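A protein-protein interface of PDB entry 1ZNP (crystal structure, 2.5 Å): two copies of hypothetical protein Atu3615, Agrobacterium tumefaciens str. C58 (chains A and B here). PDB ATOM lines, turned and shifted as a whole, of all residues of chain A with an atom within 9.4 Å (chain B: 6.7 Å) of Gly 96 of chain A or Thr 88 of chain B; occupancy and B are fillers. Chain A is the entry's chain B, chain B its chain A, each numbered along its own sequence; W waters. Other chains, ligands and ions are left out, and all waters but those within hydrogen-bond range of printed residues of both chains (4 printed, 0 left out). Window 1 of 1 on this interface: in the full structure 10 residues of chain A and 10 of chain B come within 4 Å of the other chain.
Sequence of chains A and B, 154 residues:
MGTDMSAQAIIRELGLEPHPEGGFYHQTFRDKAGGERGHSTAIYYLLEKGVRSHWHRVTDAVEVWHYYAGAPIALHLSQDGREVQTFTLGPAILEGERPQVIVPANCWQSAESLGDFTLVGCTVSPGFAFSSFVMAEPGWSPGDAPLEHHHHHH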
ATOM      1  N   PRO A  72     -10.236   1.357 -21.959  1.00  0.00           N
ATOM      2  CA  PRO A  72     -11.549   1.654 -22.521  1.00  0.00           C
ATOM      3  C   PRO A  72     -11.792   0.738 -23.702  1.00  0.00           C
ATOM      4  O   PRO A  72     -10.903   0.005 -24.132  1.00  0.00           O
ATOM      5  CB  PRO A  72     -11.421   3.109 -22.947  1.00  0.00           C
ATOM      6  CG  PRO A  72     -10.005   3.180 -23.398  1.00  0.00           C
ATOM      7  CD  PRO A  72      -9.285   2.439 -22.270  1.00  0.00           C
ATOM      8  N   ILE A  73     -12.999   0.804 -24.234  1.00  0.00           N
ATOM      9  CA  ILE A  73     -13.377  -0.025 -25.359  1.00  0.00           C
ATOM     10  C   ILE A  73     -13.849   0.798 -26.537  1.00  0.00           C
ATOM     11  O   ILE A  73     -14.356   1.901 -26.369  1.00  0.00           O
ATOM     12  CB  ILE A  73     -14.511  -0.988 -24.958  1.00  0.00           C
ATOM     13  CG1 ILE A  73     -13.920  -2.225 -24.296  1.00  0.00           C
ATOM     14  CG2 ILE A  73     -15.351  -1.357 -26.167  1.00  0.00           C
ATOM     15  CD1 ILE A  73     -14.940  -3.319 -24.053  1.00  0.00           C
ATOM     16  N   GLN A  85     -21.226   3.963 -36.223  1.00  0.00           N
ATOM     17  CA  GLN A  85     -20.746   4.981 -35.284  1.00  0.00           C
ATOM     18  C   GLN A  85     -19.790   4.332 -34.276  1.00  0.00           C
ATOM     19  O   GLN A  85     -20.074   3.268 -33.745  1.00  0.00           O
ATOM     20  CB  GLN A  85     -21.932   5.582 -34.533  1.00  0.00           C
ATOM     21  CG  GLN A  85     -23.168   5.738 -35.399  1.00  0.00           C
ATOM     22  CD  GLN A  85     -24.419   5.945 -34.578  1.00  0.00           C
ATOM     23  OE1 GLN A  85     -24.618   7.012 -33.987  1.00  0.00           O
ATOM     24  NE2 GLN A  85     -25.270   4.916 -34.526  1.00  0.00           N
ATOM     25  N   THR A  86     -18.663   4.978 -34.008  1.00  0.00           N
ATOM     26  CA  THR A  86     -17.692   4.420 -33.082  1.00  0.00           C
ATOM     27  C   THR A  86     -17.631   5.204 -31.792  1.00  0.00           C
ATOM     28  O   THR A  86     -17.371   6.408 -31.779  1.00  0.00           O
ATOM     29  CB  THR A  86     -16.291   4.351 -33.720  1.00  0.00           C
ATOM     30  OG1 THR A  86     -16.360   3.539 -34.900  1.00  0.00           O
ATOM     31  CG2 THR A  86     -15.273   3.733 -32.752  1.00  0.00           C
ATOM     32  N   PHE A  87     -17.856   4.492 -30.697  1.00  0.00           N
ATOM     33  CA  PHE A  87     -17.883   5.086 -29.372  1.00  0.00           C
ATOM     34  C   PHE A  87     -16.705   4.582 -28.546  1.00  0.00           C
ATOM     35  O   PHE A  87     -16.269   3.437 -28.699  1.00  0.00           O
ATOM     36  CB  PHE A  87     -19.194   4.680 -28.688  1.00  0.00           C
ATOM     37  CG  PHE A  87     -19.812   5.753 -27.849  1.00  0.00           C
ATOM     38  CD1 PHE A  87     -19.095   6.351 -26.796  1.00  0.00           C
ATOM     39  CD2 PHE A  87     -21.131   6.149 -28.073  1.00  0.00           C
ATOM     40  CE1 PHE A  87     -19.684   7.329 -25.974  1.00  0.00           C
ATOM     41  CE2 PHE A  87     -21.739   7.129 -27.256  1.00  0.00           C
ATOM     42  CZ  PHE A  87     -21.011   7.722 -26.201  1.00  0.00           C
ATOM     43  N   THR A  88     -16.172   5.438 -27.686  1.00  0.00           N
ATOM     44  CA  THR A  88     -15.090   5.029 -26.815  1.00  0.00           C
ATOM     45  C   THR A  88     -15.770   4.859 -25.454  1.00  0.00           C
ATOM     46  O   THR A  88     -16.178   5.824 -24.827  1.00  0.00           O
ATOM     47  CB  THR A  88     -13.970   6.094 -26.757  1.00  0.00           C
ATOM     48  OG1 THR A  88     -13.386   6.242 -28.054  1.00  0.00           O
ATOM     49  CG2 THR A  88     -12.877   5.675 -25.814  1.00  0.00           C
ATOM     50  N   LEU A  89     -15.925   3.608 -25.031  1.00  0.00           N
ATOM     51  CA  LEU A  89     -16.573   3.281 -23.766  1.00  0.00           C
ATOM     52  C   LEU A  89     -15.538   3.268 -22.643  1.00  0.00           C
ATOM     53  O   LEU A  89     -14.775   2.312 -22.489  1.00  0.00           O
ATOM     54  CB  LEU A  89     -17.247   1.909 -23.884  1.00  0.00           C
ATOM     55  CG  LEU A  89     -17.947   1.312 -22.659  1.00  0.00           C
ATOM     56  CD1 LEU A  89     -19.224   2.109 -22.327  1.00  0.00           C
ATOM     57  CD2 LEU A  89     -18.283  -0.146 -22.960  1.00  0.00           C
ATOM     58  N   GLY A  90     -15.506   4.345 -21.870  1.00  0.00           N
ATOM     59  CA  GLY A  90     -14.542   4.441 -20.796  1.00  0.00           C
ATOM     60  C   GLY A  90     -14.971   5.467 -19.774  1.00  0.00           C
ATOM     61  O   GLY A  90     -15.996   6.146 -19.956  1.00  0.00           O
ATOM     62  N   PRO A  91     -14.202   5.605 -18.681  1.00  0.00           N
ATOM     63  CA  PRO A  91     -14.488   6.549 -17.604  1.00  0.00           C
ATOM     64  C   PRO A  91     -13.893   7.944 -17.791  1.00  0.00           C
ATOM     65  O   PRO A  91     -14.256   8.872 -17.064  1.00  0.00           O
ATOM     66  CB  PRO A  91     -13.908   5.844 -16.402  1.00  0.00           C
ATOM     67  CG  PRO A  91     -12.653   5.275 -16.990  1.00  0.00           C
ATOM     68  CD  PRO A  91     -13.131   4.674 -18.275  1.00  0.00           C
ATOM     69  N   ALA A  92     -12.985   8.094 -18.751  1.00  0.00           N
ATOM     70  CA  ALA A  92     -12.344   9.390 -19.005  1.00  0.00           C
ATOM     71  C   ALA A  92     -13.319  10.429 -19.590  1.00  0.00           C
ATOM     72  O   ALA A  92     -13.163  10.896 -20.722  1.00  0.00           O
ATOM     73  CB  ALA A  92     -11.142   9.208 -19.928  1.00  0.00           C
ATOM     74  N   ILE A  93     -14.321  10.762 -18.779  1.00  0.00           N
ATOM     75  CA  ILE A  93     -15.377  11.727 -19.067  1.00  0.00           C
ATOM     76  C   ILE A  93     -14.925  13.034 -19.755  1.00  0.00           C
ATOM     77  O   ILE A  93     -15.674  13.640 -20.528  1.00  0.00           O
ATOM     78  CB  ILE A  93     -16.084  12.111 -17.736  1.00  0.00           C
ATOM     79  CG1 ILE A  93     -16.681  10.874 -17.092  1.00  0.00           C
ATOM     80  CG2 ILE A  93     -17.161  13.130 -17.973  1.00  0.00           C
ATOM     81  CD1 ILE A  93     -17.597  10.100 -18.012  1.00  0.00           C
ATOM     82  N   LEU A  94     -13.713  13.485 -19.463  1.00  0.00           N
ATOM     83  CA  LEU A  94     -13.243  14.737 -20.049  1.00  0.00           C
ATOM     84  C   LEU A  94     -12.315  14.498 -21.227  1.00  0.00           C
ATOM     85  O   LEU A  94     -11.666  15.421 -21.695  1.00  0.00           O
ATOM     86  CB  LEU A  94     -12.532  15.570 -18.981  1.00  0.00           C
ATOM     87  CG  LEU A  94     -13.331  15.735 -17.680  1.00  0.00           C
ATOM     88  CD1 LEU A  94     -12.453  16.311 -16.580  1.00  0.00           C
ATOM     89  CD2 LEU A  94     -14.534  16.615 -17.944  1.00  0.00           C
ATOM     90  N   GLU A  95     -12.287  13.256 -21.707  1.00  0.00           N
ATOM     91  CA  GLU A  95     -11.438  12.846 -22.820  1.00  0.00           C
ATOM     92  C   GLU A  95     -12.266  12.293 -23.976  1.00  0.00           C
ATOM     93  O   GLU A  95     -11.765  11.531 -24.801  1.00  0.00           O
ATOM     94  CB  GLU A  95     -10.466  11.769 -22.347  1.00  0.00           C
ATOM     95  CG  GLU A  95      -9.827  12.082 -21.017  1.00  0.00           C
ATOM     96  CD  GLU A  95      -8.655  13.015 -21.142  1.00  0.00           C
ATOM     97  OE1 GLU A  95      -7.505  12.516 -21.184  1.00  0.00           O
ATOM     98  OE2 GLU A  95      -8.884  14.241 -21.212  1.00  0.00           O
ATOM     99  N   GLY A  96     -13.539  12.658 -24.021  1.00  0.00           N
ATOM    100  CA  GLY A  96     -14.393  12.199 -25.101  1.00  0.00           C
ATOM    101  C   GLY A  96     -14.906  10.787 -24.926  1.00  0.00           C
ATOM    102  O   GLY A  96     -15.409  10.176 -25.874  1.00  0.00           O
ATOM    103  N   GLU A  97     -14.771  10.261 -23.714  1.00  0.00           N
ATOM    104  CA  GLU A  97     -15.228   8.910 -23.398  1.00  0.00           C
ATOM    105  C   GLU A  97     -16.529   8.978 -22.610  1.00  0.00           C
ATOM    106  O   GLU A  97     -16.859  10.014 -22.026  1.00  0.00           O
ATOM    107  CB  GLU A  97     -14.198   8.172 -22.534  1.00  0.00           C
ATOM    108  CG  GLU A  97     -12.952   7.669 -23.246  1.00  0.00           C
ATOM    109  CD  GLU A  97     -11.938   7.053 -22.279  1.00  0.00           C
ATOM    110  OE1 GLU A  97     -12.354   6.483 -21.253  1.00  0.00           O
ATOM    111  OE2 GLU A  97     -10.725   7.128 -22.548  1.00  0.00           O
ATOM    112  N   ARG A  98     -17.249   7.859 -22.603  1.00  0.00           N
ATOM    113  CA  ARG A  98     -18.490   7.703 -21.857  1.00  0.00           C
ATOM    114  C   ARG A  98     -18.510   6.272 -21.351  1.00  0.00           C
ATOM    115  O   ARG A  98     -18.257   5.344 -22.105  1.00  0.00           O
ATOM    116  CB  ARG A  98     -19.703   7.990 -22.739  1.00  0.00           C
ATOM    117  CG  ARG A  98     -19.944   9.486 -22.934  1.00  0.00           C
ATOM    118  CD  ARG A  98     -20.199  10.179 -21.590  1.00  0.00           C
ATOM    119  NE  ARG A  98     -20.401  11.618 -21.718  1.00  0.00           N
ATOM    120  CZ  ARG A  98     -19.427  12.529 -21.747  1.00  0.00           C
ATOM    121  NH1 ARG A  98     -19.730  13.818 -21.861  1.00  0.00           N
ATOM    122  NH2 ARG A  98     -18.156  12.166 -21.658  1.00  0.00           N
ATOM    123  N   PRO A  99     -18.799   6.073 -20.056  1.00  0.00           N
ATOM    124  CA  PRO A  99     -18.838   4.734 -19.451  1.00  0.00           C
ATOM    125  C   PRO A  99     -20.146   3.958 -19.645  1.00  0.00           C
ATOM    126  O   PRO A  99     -20.291   2.835 -19.149  1.00  0.00           O
ATOM    127  CB  PRO A  99     -18.547   5.027 -17.983  1.00  0.00           C
ATOM    128  CG  PRO A  99     -19.289   6.302 -17.774  1.00  0.00           C
ATOM    129  CD  PRO A  99     -19.018   7.114 -19.037  1.00  0.00           C
ATOM    130  N   LEU A 114      -9.178  -1.454 -26.036  1.00  0.00           N
ATOM    131  CA  LEU A 114      -8.132  -0.594 -26.547  1.00  0.00           C
ATOM    132  C   LEU A 114      -6.879  -0.816 -25.697  1.00  0.00           C
ATOM    133  O   LEU A 114      -5.917  -0.048 -25.760  1.00  0.00           O
ATOM    134  CB  LEU A 114      -8.603   0.868 -26.488  1.00  0.00           C
ATOM    135  CG  LEU A 114      -9.187   1.508 -27.768  1.00  0.00           C
ATOM    136  CD1 LEU A 114      -9.733   0.457 -28.718  1.00  0.00           C
ATOM    137  CD2 LEU A 114     -10.276   2.512 -27.392  1.00  0.00           C
ATOM    138  N   PRO B  72      -7.658  15.930 -30.837  1.00  0.00           N
ATOM    139  CA  PRO B  72      -8.998  15.459 -31.196  1.00  0.00           C
ATOM    140  C   PRO B  72     -10.051  16.310 -30.512  1.00  0.00           C
ATOM    141  O   PRO B  72      -9.730  17.179 -29.702  1.00  0.00           O
ATOM    142  CB  PRO B  72      -9.007  14.010 -30.709  1.00  0.00           C
ATOM    143  CG  PRO B  72      -7.988  14.009 -29.591  1.00  0.00           C
ATOM    144  CD  PRO B  72      -6.889  14.873 -30.156  1.00  0.00           C
ATOM    145  N   ILE B  73     -11.308  16.057 -30.836  1.00  0.00           N
ATOM    146  CA  ILE B  73     -12.404  16.803 -30.253  1.00  0.00           C
ATOM    147  C   ILE B  73     -13.434  15.869 -29.642  1.00  0.00           C
ATOM    148  O   ILE B  73     -13.558  14.711 -30.033  1.00  0.00           O
ATOM    149  CB  ILE B  73     -13.106  17.692 -31.334  1.00  0.00           C
ATOM    150  CG1 ILE B  73     -12.577  19.126 -31.256  1.00  0.00           C
ATOM    151  CG2 ILE B  73     -14.632  17.645 -31.178  1.00  0.00           C
ATOM    152  CD1 ILE B  73     -13.196  20.064 -32.276  1.00  0.00           C
ATOM    153  N   ALA B  74     -14.159  16.381 -28.655  1.00  0.00           N
ATOM    154  CA  ALA B  74     -15.224  15.612 -28.046  1.00  0.00           C
ATOM    155  C   ALA B  74     -16.493  16.249 -28.618  1.00  0.00           C
ATOM    156  O   ALA B  74     -16.786  17.423 -28.362  1.00  0.00           O
ATOM    157  CB  ALA B  74     -15.185  15.748 -26.563  1.00  0.00           C
ATOM    158  N   LEU B  75     -17.209  15.477 -29.431  1.00  0.00           N
ATOM    159  CA  LEU B  75     -18.441  15.930 -30.066  1.00  0.00           C
ATOM    160  C   LEU B  75     -19.609  15.252 -29.359  1.00  0.00           C
ATOM    161  O   LEU B  75     -19.655  14.026 -29.256  1.00  0.00           O
ATOM    162  CB  LEU B  75     -18.427  15.565 -31.550  1.00  0.00           C
ATOM    163  CG  LEU B  75     -19.520  16.180 -32.419  1.00  0.00           C
ATOM    164  CD1 LEU B  75     -19.414  17.680 -32.417  1.00  0.00           C
ATOM    165  CD2 LEU B  75     -19.373  15.674 -33.832  1.00  0.00           C
ATOM    166  N   HIS B  76     -20.540  16.059 -28.862  1.00  0.00           N
ATOM    167  CA  HIS B  76     -21.698  15.562 -28.135  1.00  0.00           C
ATOM    168  C   HIS B  76     -22.970  15.760 -28.942  1.00  0.00           C
ATOM    169  O   HIS B  76     -23.229  16.856 -29.434  1.00  0.00           O
ATOM    170  CB  HIS B  76     -21.803  16.300 -26.804  1.00  0.00           C
ATOM    171  CG  HIS B  76     -20.510  16.358 -26.044  1.00  0.00           C
ATOM    172  ND1 HIS B  76     -19.957  15.257 -25.421  1.00  0.00           N
ATOM    173  CD2 HIS B  76     -19.652  17.384 -25.825  1.00  0.00           C
ATOM    174  CE1 HIS B  76     -18.816  15.604 -24.852  1.00  0.00           C
ATOM    175  NE2 HIS B  76     -18.608  16.886 -25.081  1.00  0.00           N
ATOM    176  N   THR B  86     -21.476  10.670 -27.226  1.00  0.00           N
ATOM    177  CA  THR B  86     -20.237  11.423 -27.363  1.00  0.00           C
ATOM    178  C   THR B  86     -19.229  10.679 -28.216  1.00  0.00           C
ATOM    179  O   THR B  86     -18.877   9.531 -27.938  1.00  0.00           O
ATOM    180  CB  THR B  86     -19.617  11.719 -25.982  1.00  0.00           C
ATOM    181  OG1 THR B  86     -20.520  12.534 -25.224  1.00  0.00           O
ATOM    182  CG2 THR B  86     -18.276  12.450 -26.137  1.00  0.00           C
ATOM    183  N   PHE B  87     -18.764  11.343 -29.263  1.00  0.00           N
ATOM    184  CA  PHE B  87     -17.800  10.737 -30.161  1.00  0.00           C
ATOM    185  C   PHE B  87     -16.500  11.513 -30.122  1.00  0.00           C
ATOM    186  O   PHE B  87     -16.500  12.736 -30.038  1.00  0.00           O
ATOM    187  CB  PHE B  87     -18.357  10.727 -31.590  1.00  0.00           C
ATOM    188  CG  PHE B  87     -19.710  10.094 -31.700  1.00  0.00           C
ATOM    189  CD1 PHE B  87     -19.868   8.717 -31.521  1.00  0.00           C
ATOM    190  CD2 PHE B  87     -20.838  10.873 -31.942  1.00  0.00           C
ATOM    191  CE1 PHE B  87     -21.135   8.126 -31.582  1.00  0.00           C
ATOM    192  CE2 PHE B  87     -22.106  10.292 -32.005  1.00  0.00           C
ATOM    193  CZ  PHE B  87     -22.254   8.918 -31.826  1.00  0.00           C
ATOM    194  N   THR B  88     -15.389  10.797 -30.153  1.00  0.00           N
ATOM    195  CA  THR B  88     -14.100  11.449 -30.168  1.00  0.00           C
ATOM    196  C   THR B  88     -13.755  11.613 -31.644  1.00  0.00           C
ATOM    197  O   THR B  88     -13.529  10.640 -32.361  1.00  0.00           O
ATOM    198  CB  THR B  88     -13.029  10.612 -29.440  1.00  0.00           C
ATOM    199  OG1 THR B  88     -13.387  10.499 -28.055  1.00  0.00           O
ATOM    200  CG2 THR B  88     -11.676  11.297 -29.510  1.00  0.00           C
ATOM    201  N   LEU B  89     -13.769  12.858 -32.092  1.00  0.00           N
ATOM    202  CA  LEU B  89     -13.472  13.199 -33.472  1.00  0.00           C
ATOM    203  C   LEU B  89     -11.978  13.414 -33.582  1.00  0.00           C
ATOM    204  O   LEU B  89     -11.439  14.312 -32.949  1.00  0.00           O
ATOM    205  CB  LEU B  89     -14.194  14.488 -33.849  1.00  0.00           C
ATOM    206  CG  LEU B  89     -13.922  15.030 -35.251  1.00  0.00           C
ATOM    207  CD1 LEU B  89     -14.522  14.097 -36.286  1.00  0.00           C
ATOM    208  CD2 LEU B  89     -14.506  16.428 -35.367  1.00  0.00           C
ATOM    209  N   GLY B  90     -11.313  12.590 -34.386  1.00  0.00           N
ATOM    210  CA  GLY B  90      -9.879  12.713 -34.541  1.00  0.00           C
ATOM    211  C   GLY B  90      -9.328  11.694 -35.511  1.00  0.00           C
ATOM    212  O   GLY B  90     -10.082  10.909 -36.079  1.00  0.00           O
ATOM    213  N   PRO B  91      -8.005  11.670 -35.711  1.00  0.00           N
ATOM    214  CA  PRO B  91      -7.385  10.725 -36.633  1.00  0.00           C
ATOM    215  C   PRO B  91      -6.923   9.383 -36.055  1.00  0.00           C
ATOM    216  O   PRO B  91      -6.610   8.475 -36.815  1.00  0.00           O
ATOM    217  CB  PRO B  91      -6.219  11.531 -37.184  1.00  0.00           C
ATOM    218  CG  PRO B  91      -5.743  12.252 -35.959  1.00  0.00           C
ATOM    219  CD  PRO B  91      -7.042  12.715 -35.305  1.00  0.00           C
ATOM    220  N   GLU B  95      -7.787   3.836 -31.949  1.00  0.00           N
ATOM    221  CA  GLU B  95      -7.985   4.118 -30.531  1.00  0.00           C
ATOM    222  C   GLU B  95      -9.367   4.704 -30.219  1.00  0.00           C
ATOM    223  O   GLU B  95      -9.532   5.476 -29.276  1.00  0.00           O
ATOM    224  CB  GLU B  95      -6.877   5.070 -30.069  1.00  0.00           C
ATOM    225  CG  GLU B  95      -5.485   4.657 -30.569  1.00  0.00           C
ATOM    226  CD  GLU B  95      -4.434   5.747 -30.398  1.00  0.00           C
ATOM    227  OE1 GLU B  95      -3.312   5.585 -30.941  1.00  0.00           O
ATOM    228  OE2 GLU B  95      -4.727   6.768 -29.726  1.00  0.00           O
ATOM    229  N   GLY B  96     -10.365   4.341 -31.013  1.00  0.00           N
ATOM    230  CA  GLY B  96     -11.707   4.835 -30.763  1.00  0.00           C
ATOM    231  C   GLY B  96     -12.039   6.167 -31.408  1.00  0.00           C
ATOM    232  O   GLY B  96     -13.063   6.760 -31.091  1.00  0.00           O
ATOM    233  N   GLU B  97     -11.191   6.631 -32.317  1.00  0.00           N
ATOM    234  CA  GLU B  97     -11.420   7.913 -32.975  1.00  0.00           C
ATOM    235  C   GLU B  97     -11.887   7.761 -34.414  1.00  0.00           C
ATOM    236  O   GLU B  97     -11.602   6.762 -35.077  1.00  0.00           O
ATOM    237  CB  GLU B  97     -10.137   8.748 -32.961  1.00  0.00           C
ATOM    238  CG  GLU B  97      -9.972   9.655 -31.741  1.00  0.00           C
ATOM    239  CD  GLU B  97      -8.568  10.264 -31.630  1.00  0.00           C
ATOM    240  OE1 GLU B  97      -8.000  10.672 -32.676  1.00  0.00           O
ATOM    241  OE2 GLU B  97      -8.042  10.341 -30.491  1.00  0.00           O
ATOM    242  N   ARG B  98     -12.613   8.765 -34.886  1.00  0.00           N
ATOM    243  CA  ARG B  98     -13.101   8.804 -36.258  1.00  0.00           C
ATOM    244  C   ARG B  98     -12.983  10.261 -36.668  1.00  0.00           C
ATOM    245  O   ARG B  98     -13.415  11.148 -35.942  1.00  0.00           O
ATOM    246  CB  ARG B  98     -14.550   8.316 -36.350  1.00  0.00           C
ATOM    247  CG  ARG B  98     -14.703   6.787 -36.169  1.00  0.00           C
ATOM    248  CD  ARG B  98     -14.018   6.070 -37.322  1.00  0.00           C
ATOM    249  NE  ARG B  98     -13.992   4.612 -37.226  1.00  0.00           N
ATOM    250  CZ  ARG B  98     -13.128   3.905 -36.496  1.00  0.00           C
ATOM    251  NH1 ARG B  98     -13.189   2.580 -36.496  1.00  0.00           N
ATOM    252  NH2 ARG B  98     -12.204   4.511 -35.774  1.00  0.00           N
ATOM    253  N   PRO B  99     -12.354  10.525 -37.822  1.00  0.00           N
ATOM    254  CA  PRO B  99     -12.174  11.890 -38.318  1.00  0.00           C
ATOM    255  C   PRO B  99     -13.409  12.434 -39.019  1.00  0.00           C
ATOM    256  O   PRO B  99     -13.402  13.538 -39.541  1.00  0.00           O
ATOM    257  CB  PRO B  99     -10.979  11.760 -39.260  1.00  0.00           C
ATOM    258  CG  PRO B  99     -11.208  10.392 -39.876  1.00  0.00           C
ATOM    259  CD  PRO B  99     -11.660   9.545 -38.680  1.00  0.00           C
ATOM    260  N   VAL B 101     -17.780  12.505 -38.510  1.00  0.00           N
ATOM    261  CA  VAL B 101     -18.956  12.161 -37.713  1.00  0.00           C
ATOM    262  C   VAL B 101     -20.175  12.935 -38.229  1.00  0.00           C
ATOM    263  O   VAL B 101     -20.110  14.144 -38.499  1.00  0.00           O
ATOM    264  CB  VAL B 101     -18.728  12.432 -36.207  1.00  0.00           C
ATOM    265  CG1 VAL B 101     -18.039  13.749 -36.024  1.00  0.00           C
ATOM    266  CG2 VAL B 101     -20.047  12.445 -35.473  1.00  0.00           C
ATOM    267  N   GLU B 112     -15.862  20.435 -27.897  1.00  0.00           N
ATOM    268  CA  GLU B 112     -14.750  21.086 -27.230  1.00  0.00           C
ATOM    269  C   GLU B 112     -13.463  20.411 -27.686  1.00  0.00           C
ATOM    270  O   GLU B 112     -13.448  19.214 -27.979  1.00  0.00           O
ATOM    271  CB  GLU B 112     -14.894  20.986 -25.705  1.00  0.00           C
ATOM    272  CG  GLU B 112     -14.978  19.568 -25.197  1.00  0.00           C
ATOM    273  CD  GLU B 112     -16.382  19.154 -24.738  1.00  0.00           C
ATOM    274  OE1 GLU B 112     -16.501  18.024 -24.198  1.00  0.00           O
ATOM    275  OE2 GLU B 112     -17.350  19.939 -24.907  1.00  0.00           O
ATOM    276  N   LEU B 114      -9.742  18.895 -27.200  1.00  0.00           N
ATOM    277  CA  LEU B 114      -9.121  18.170 -26.102  1.00  0.00           C
ATOM    278  C   LEU B 114      -7.659  18.558 -25.924  1.00  0.00           C
ATOM    279  O   LEU B 114      -6.927  17.935 -25.162  1.00  0.00           O
ATOM    280  CB  LEU B 114      -9.248  16.665 -26.331  1.00  0.00           C
ATOM    281  CG  LEU B 114     -10.698  16.213 -26.499  1.00  0.00           C
ATOM    282  CD1 LEU B 114     -10.763  14.715 -26.710  1.00  0.00           C
ATOM    283  CD2 LEU B 114     -11.500  16.600 -25.272  1.00  0.00           C
HETATM  284  O   HOH W   1     -11.589   9.293 -26.270  1.00  0.00           O
HETATM  285  O   HOH W   2     -22.927  11.288 -24.088  1.00  0.00           O
HETATM  286  O   HOH W   3     -17.235   4.604 -37.129  1.00  0.00           O
HETATM  287  O   HOH W   4     -11.014   7.867 -28.647  1.00  0.00           O
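The backbone carbonyl oxygen (O) of Gly 96 of chain A lies within hydrogen-bond range of the side-chain hydroxyl (OG1) of Thr 88 of chain B (3.0 Å). The side-chain hydroxyl (OG1) of Thr 88 of chain A lies within hydrogen-bond range of the backbone carbonyl oxygen (O) of Gly 96 of chain B (3.1 Å). OG1 of Thr 86 of chain A is in hydrogen-bond range of NE of Arg 98 of chain B (3.5 Å).
O of Pro 72 of chain B is in hydrogen-bond range of N of Leu 114 of chain B. The backbone NH of Ala 74 of chain B is in hydrogen-bond range of the backbone carbonyl oxygen of Glu 112 of chain B, 3.0 Å away. OG1 of Thr 86 of chain B lies within hydrogen-bond range of ND1 of His 76 of chain B (2.8 Å). A ring nitrogen (NE2) of His 76 of chain B sits at hydrogen-bond distance from the side-chain carboxylate (OE1) of Glu 112 of chain B. O of Thr 88 of chain B sits at hydrogen-bond distance from N of Arg 98 of chain B. N of Gly 90 of chain A sits at hydrogen-bond distance from O of Arg 98 of chain A (2.9 Å).
CZ of Phe 87 of chain B touches OE1 of Gln 85 of chain A, at 3.7 Å. O of Thr 86 of chain A touches CD1 of Phe 87 of chain B, 3.4 Å away. Phe 87 of chain A touches Thr 86 of chain B. Leu 94 of chain A touches Leu 114 of chain B (O to CD2, 3.8 Å). Thr 88 of chain B touches Glu 95 of chain A (OG1 to O, 3.8 Å). O of Glu 95 of chain A touches CD1 of Leu 114 of chain B, 3.8 Å away. Gly 96 of chain A touches Ala 74 of chain B. Thr 86 of chain B touches Gly 96 of chain A. NH1 of Arg 98 of chain A touches CE1 of His 76 of chain B, 3.6 Å away. NE of Arg 98 of chain A touches OG1 of Thr 86 of chain B, at 3.6 Å.
Ile 73 of chain A touches none of the printed residues of chain B. Of the printed residues of chain B, Leu 94 of chain A touches Leu 114. Printed residues of chain B within 4 Å of Glu 95 of chain A: Thr 88 (3.8 Å) and Leu 114 (3.8 Å). Of chain B, only Ala 74, Thr 86 and Thr 88 come within 4 Å of Gly 96 of chain A. Printed residues of chain A within 4 Å of Ala 74 of chain B: Gly 96 (3.9 Å). Of chain A, only Glu 95 and Gly 96 come within 4 Å of Thr 88 of chain B. No residue of chain A comes within 4 Å of Glu 97 of chain B. Printed residues of chain A within 4 Å of Leu 114 of chain B: Leu 94 (3.8 Å) and Glu 95 (3.8 Å). The nearest residue of chain A that does not touch Thr 88 of chain B is Thr 88 of chain A (4.3 Å).
Of the 18 printed residues of chain A, 9 touch a printed residue of chain B. Hydrophobic or aromatic side chains of chain A that line the printed part of chain B: Phe 87 and Leu 114. Along chain A the printed residues that touch a printed residue of chain B span positions 85 to 114. Hydrophobic or aromatic side chains of chain B that line the printed part of chain A: Ala 74, His 76, Phe 87 and Leu 114. Among the printed residues, no Asp or Glu carboxylate lies within 4 Å of a Lys or Arg side-chain nitrogen of the other chain.
Thr 86 of chain A touches Arg 98 of chain B, and with the chains exchanged Arg 98 of chain A touches Thr 86 of chain B. Thr 88 of chain A touches Gly 96 of chain B, and with the chains exchanged Gly 96 of chain A touches Thr 88 of chain B. Glu 95 of chain A touches Leu 114 of chain B, and with the chains exchanged Leu 114 of chain A touches Glu 95 of chain B. Gly 96 of chain A touches Thr 86 of chain B, but with the chains exchanged Thr 86 of chain A does not touch Gly 96 of chain B (4.1 Å).
Water W3 lies within hydrogen-bond range of OG1 of Thr 86 of chain A (2.6 Å) and NE of Arg 98 of chain B (3.2 Å). Water W1 bridges the backbone carbonyl oxygen of Glu 95 of chain A (2.7 Å) and the side-chain hydroxyl of Thr 88 of chain B (2.8 Å). Water W4 lies within hydrogen-bond range of O of Glu 95 of chain B (2.9 Å), OG1 of Thr 88 of chain A (2.9 Å) and O of Gly 96 of chain B (3.4 Å). Water W2 bridges the side-chain hydroxyl (OG1) of Thr 86 of chain B (2.9 Å) and the guanidinium group (NE) of Arg 98 of chain A (3.5 Å).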
